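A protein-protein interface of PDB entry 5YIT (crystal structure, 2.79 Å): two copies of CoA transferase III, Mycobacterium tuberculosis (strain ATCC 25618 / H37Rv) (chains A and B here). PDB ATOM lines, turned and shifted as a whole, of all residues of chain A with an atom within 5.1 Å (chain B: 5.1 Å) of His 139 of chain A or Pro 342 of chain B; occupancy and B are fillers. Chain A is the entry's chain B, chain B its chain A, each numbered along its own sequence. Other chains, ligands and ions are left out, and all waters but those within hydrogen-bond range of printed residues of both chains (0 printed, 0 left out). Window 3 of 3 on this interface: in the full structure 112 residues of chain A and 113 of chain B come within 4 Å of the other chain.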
ATOM      1  N   TYR A 133       5.342 -30.328   0.245  1.00  0.00           N
ATOM      2  CA  TYR A 133       4.827 -30.167  -1.107  1.00  0.00           C
ATOM      3  C   TYR A 133       5.582 -30.938  -2.200  1.00  0.00           C
ATOM      4  O   TYR A 133       5.084 -31.121  -3.314  1.00  0.00           O
ATOM      5  CB  TYR A 133       4.789 -28.704  -1.412  1.00  0.00           C
ATOM      6  CG  TYR A 133       3.859 -27.939  -0.520  1.00  0.00           C
ATOM      7  CD1 TYR A 133       2.455 -27.969  -0.707  1.00  0.00           C
ATOM      8  CD2 TYR A 133       4.364 -27.143   0.488  1.00  0.00           C
ATOM      9  CE1 TYR A 133       1.604 -27.213   0.099  1.00  0.00           C
ATOM     10  CE2 TYR A 133       3.525 -26.372   1.288  1.00  0.00           C
ATOM     11  CZ  TYR A 133       2.154 -26.420   1.112  1.00  0.00           C
ATOM     12  OH  TYR A 133       1.345 -25.694   1.965  1.00  0.00           O
ATOM     13  N   GLY A 137      10.123 -28.382  -8.500  1.00  0.00           N
ATOM     14  CA  GLY A 137       9.699 -27.084  -8.988  1.00  0.00           C
ATOM     15  C   GLY A 137       9.477 -26.013  -7.931  1.00  0.00           C
ATOM     16  O   GLY A 137       9.583 -26.265  -6.739  1.00  0.00           O
ATOM     17  N   PRO A 138       9.197 -24.797  -8.380  1.00  0.00           N
ATOM     18  CA  PRO A 138       9.090 -23.602  -7.546  1.00  0.00           C
ATOM     19  C   PRO A 138       7.890 -23.573  -6.609  1.00  0.00           C
ATOM     20  O   PRO A 138       8.010 -23.073  -5.493  1.00  0.00           O
ATOM     21  CB  PRO A 138       9.026 -22.444  -8.550  1.00  0.00           C
ATOM     22  CG  PRO A 138       8.884 -23.077  -9.885  1.00  0.00           C
ATOM     23  CD  PRO A 138       9.394 -24.474  -9.789  1.00  0.00           C
ATOM     24  N   HIS A 139       6.753 -24.098  -7.042  1.00  0.00           N
ATOM     25  CA  HIS A 139       5.578 -24.108  -6.184  1.00  0.00           C
ATOM     26  C   HIS A 139       5.704 -25.116  -5.028  1.00  0.00           C
ATOM     27  O   HIS A 139       5.108 -24.922  -4.002  1.00  0.00           O
ATOM     28  CB  HIS A 139       4.347 -24.373  -7.008  1.00  0.00           C
ATOM     29  CG  HIS A 139       4.117 -23.369  -8.095  1.00  0.00           C
ATOM     30  ND1 HIS A 139       4.446 -23.598  -9.419  1.00  0.00           N
ATOM     31  CD2 HIS A 139       3.571 -22.130  -8.054  1.00  0.00           C
ATOM     32  CE1 HIS A 139       4.119 -22.539 -10.143  1.00  0.00           C
ATOM     33  NE2 HIS A 139       3.583 -21.636  -9.339  1.00  0.00           N
ATOM     34  N   GLY A 140       6.509 -26.164  -5.183  1.00  0.00           N
ATOM     35  CA  GLY A 140       6.732 -27.127  -4.112  1.00  0.00           C
ATOM     36  C   GLY A 140       7.927 -26.818  -3.222  1.00  0.00           C
ATOM     37  O   GLY A 140       8.319 -27.641  -2.368  1.00  0.00           O
ATOM     38  N   SER A 141       8.514 -25.639  -3.440  1.00  0.00           N
ATOM     39  CA  SER A 141       9.727 -25.204  -2.733  1.00  0.00           C
ATOM     40  C   SER A 141       9.479 -24.937  -1.245  1.00  0.00           C
ATOM     41  O   SER A 141      10.385 -25.110  -0.428  1.00  0.00           O
ATOM     42  CB  SER A 141      10.310 -23.974  -3.403  1.00  0.00           C
ATOM     43  N   ARG A 142       8.249 -24.544  -0.917  1.00  0.00           N
ATOM     44  CA  ARG A 142       7.852 -24.114   0.413  1.00  0.00           C
ATOM     45  C   ARG A 142       7.925 -25.101   1.585  1.00  0.00           C
ATOM     46  O   ARG A 142       8.110 -26.305   1.420  1.00  0.00           O
ATOM     47  CB  ARG A 142       6.463 -23.541   0.328  1.00  0.00           C
ATOM     48  CG  ARG A 142       6.323 -22.578  -0.829  1.00  0.00           C
ATOM     49  CD  ARG A 142       4.909 -22.069  -1.002  1.00  0.00           C
ATOM     50  NE  ARG A 142       4.067 -23.013  -1.735  1.00  0.00           N
ATOM     51  CZ  ARG A 142       2.808 -23.315  -1.404  1.00  0.00           C
ATOM     52  NH1 ARG A 142       2.254 -22.747  -0.339  1.00  0.00           N
ATOM     53  NH2 ARG A 142       2.113 -24.184  -2.132  1.00  0.00           N
ATOM     54  N   ASP B 340      -6.805 -27.483 -11.038  1.00  0.00           N
ATOM     55  CA  ASP B 340      -6.278 -26.487 -11.965  1.00  0.00           C
ATOM     56  C   ASP B 340      -5.197 -25.628 -11.347  1.00  0.00           C
ATOM     57  O   ASP B 340      -4.915 -24.559 -11.867  1.00  0.00           O
ATOM     58  CB  ASP B 340      -7.384 -25.571 -12.468  1.00  0.00           C
ATOM     59  CG  ASP B 340      -8.361 -26.289 -13.326  1.00  0.00           C
ATOM     60  OD1 ASP B 340      -7.892 -26.981 -14.266  1.00  0.00           O
ATOM     61  OD2 ASP B 340      -9.587 -26.176 -13.042  1.00  0.00           O
ATOM     62  N   THR B 341      -4.595 -26.072 -10.252  1.00  0.00           N
ATOM     63  CA  THR B 341      -3.483 -25.329  -9.672  1.00  0.00           C
ATOM     64  C   THR B 341      -2.170 -25.747 -10.287  1.00  0.00           C
ATOM     65  O   THR B 341      -2.053 -26.864 -10.766  1.00  0.00           O
ATOM     66  CB  THR B 341      -3.335 -25.523  -8.152  1.00  0.00           C
ATOM     67  OG1 THR B 341      -3.362 -26.910  -7.838  1.00  0.00           O
ATOM     68  CG2 THR B 341      -4.438 -24.853  -7.435  1.00  0.00           C
ATOM     69  N   PRO B 342      -1.185 -24.836 -10.273  1.00  0.00           N
ATOM     70  CA  PRO B 342       0.154 -25.110 -10.741  1.00  0.00           C
ATOM     71  C   PRO B 342       0.829 -26.126  -9.866  1.00  0.00           C
ATOM     72  O   PRO B 342       1.610 -26.890 -10.369  1.00  0.00           O
ATOM     73  CB  PRO B 342       0.870 -23.747 -10.664  1.00  0.00           C
ATOM     74  CG  PRO B 342      -0.059 -22.822  -9.971  1.00  0.00           C
ATOM     75  CD  PRO B 342      -1.434 -23.394 -10.095  1.00  0.00           C
ATOM     76  N   LEU B 343       0.517 -26.124  -8.577  1.00  0.00           N
ATOM     77  CA  LEU B 343       1.143 -27.016  -7.651  1.00  0.00           C
ATOM     78  C   LEU B 343       0.776 -28.466  -7.953  1.00  0.00           C
ATOM     79  O   LEU B 343       1.588 -29.367  -7.821  1.00  0.00           O
ATOM     80  CB  LEU B 343       0.725 -26.634  -6.255  1.00  0.00           C
ATOM     81  CG  LEU B 343       1.245 -27.594  -5.210  1.00  0.00           C
ATOM     82  CD1 LEU B 343       2.768 -27.589  -5.201  1.00  0.00           C
ATOM     83  CD2 LEU B 343       0.688 -27.145  -3.879  1.00  0.00           C
ATOM     84  N   PHE B 344      -0.467 -28.682  -8.320  1.00  0.00           N
ATOM     85  CA  PHE B 344      -0.956 -29.990  -8.688  1.00  0.00           C
ATOM     86  C   PHE B 344      -0.261 -30.474  -9.975  1.00  0.00           C
ATOM     87  O   PHE B 344       0.043 -31.654 -10.115  1.00  0.00           O
ATOM     88  CB  PHE B 344      -2.446 -29.828  -8.921  1.00  0.00           C
ATOM     89  CG  PHE B 344      -3.206 -31.078  -8.902  1.00  0.00           C
ATOM     90  CD1 PHE B 344      -3.625 -31.614  -7.689  1.00  0.00           C
ATOM     91  CD2 PHE B 344      -3.544 -31.726 -10.104  1.00  0.00           C
ATOM     92  CE1 PHE B 344      -4.358 -32.801  -7.668  1.00  0.00           C
ATOM     93  CE2 PHE B 344      -4.281 -32.895 -10.099  1.00  0.00           C
ATOM     94  CZ  PHE B 344      -4.697 -33.445  -8.874  1.00  0.00           C
ATOM     95  N   ALA B 345      -0.044 -29.545 -10.908  1.00  0.00           N
ATOM     96  CA  ALA B 345       0.522 -29.861 -12.196  1.00  0.00           C
ATOM     97  C   ALA B 345       1.984 -30.233 -12.056  1.00  0.00           C
ATOM     98  O   ALA B 345       2.511 -31.075 -12.775  1.00  0.00           O
ATOM     99  CB  ALA B 345       0.382 -28.666 -13.103  1.00  0.00           C
ATOM    100  N   GLU B 346       2.629 -29.555 -11.126  1.00  0.00           N
ATOM    101  CA  GLU B 346       4.034 -29.675 -10.842  1.00  0.00           C
ATOM    102  C   GLU B 346       4.373 -31.046 -10.283  1.00  0.00           C
ATOM    103  O   GLU B 346       5.448 -31.555 -10.541  1.00  0.00           O
ATOM    104  CB  GLU B 346       4.352 -28.611  -9.816  1.00  0.00           C
ATOM    105  CG  GLU B 346       5.791 -28.285  -9.635  1.00  0.00           C
ATOM    106  CD  GLU B 346       5.958 -26.914  -9.020  1.00  0.00           C
ATOM    107  OE1 GLU B 346       6.426 -26.847  -7.873  1.00  0.00           O
ATOM    108  OE2 GLU B 346       5.609 -25.905  -9.682  1.00  0.00           O
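No position is printed for both chains.
Of chain B, only Pro 342 (3.5 Å), Leu 343 (3.7 Å) and Glu 346 (2.6 Å) come within 4 Å of His 139 of chain A.
Pro 342 of chain B touches one residue of chain A.
Printed residues of chain B within 4 Å of Tyr 133 of chain A: Leu 343.
Of the printed residues of chain A, Glu 346 of chain B touches Gly 137, Pro 138, His 139 and Gly 140.
Printed residues of chain B within 4 Å of Pro 138 of chain A: Glu 346 (3.5 Å).
Thr 341 of chain B touches none of the printed residues of chain A.
The nearest printed residue of chain B that does not touch His 139 of chain A is Phe 344 of chain B (6.6 Å).
The nearest printed residue of chain A that does not touch Glu 346 of chain B is Ser 141 of chain A (5.0 Å).
Among the printed residues, merely in contact across the chains: Tyr 133 of chain A with Leu 343 of chain B (3.7 Å), His 139 of chain A with Pro 342 of chain B (3.5 Å), His 139 of chain A with Leu 343 of chain B (3.7 Å) and Arg 142 of chain A with Leu 343 of chain B (3.7 Å).
Of the 7 printed residues of chain A, 6 touch a printed residue of chain B.
Of the 7 printed residues of chain B, 3 touch a printed residue of chain A.
Hydrophobic or aromatic side chains of chain B within 4 Å of the printed part of chain A: Pro 342 and Leu 343.
Along chain B the printed residues that touch a printed residue of chain A span positions 342 to 346.
Among the printed residues, no Asp or Glu carboxylate lies within 4 Å of a Lys or Arg side-chain nitrogen of the other chain.
NE of Arg 142 of chain A is in hydrogen-bond range of O of His 139 of chain A (3.1 Å).
The side-chain carboxylate (OE2) of Glu 346 of chain B sits at hydrogen-bond distance from a ring nitrogen (ND1) of His 139 of chain A, 2.6 Å away.
The backbone NH (N) of Gly 140 of chain A lies within hydrogen-bond range of the side-chain carboxylate (OE1) of Glu 346 of chain B, 2.8 Å away.
The backbone carbonyl oxygen (O) of Gly 137 of chain A lies close to the side-chain carboxylate (OE1) of Glu 346 of chain B.
OE1 of Glu 346 of chain B lies close to N of Pro 138 of chain A (3.5 Å).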
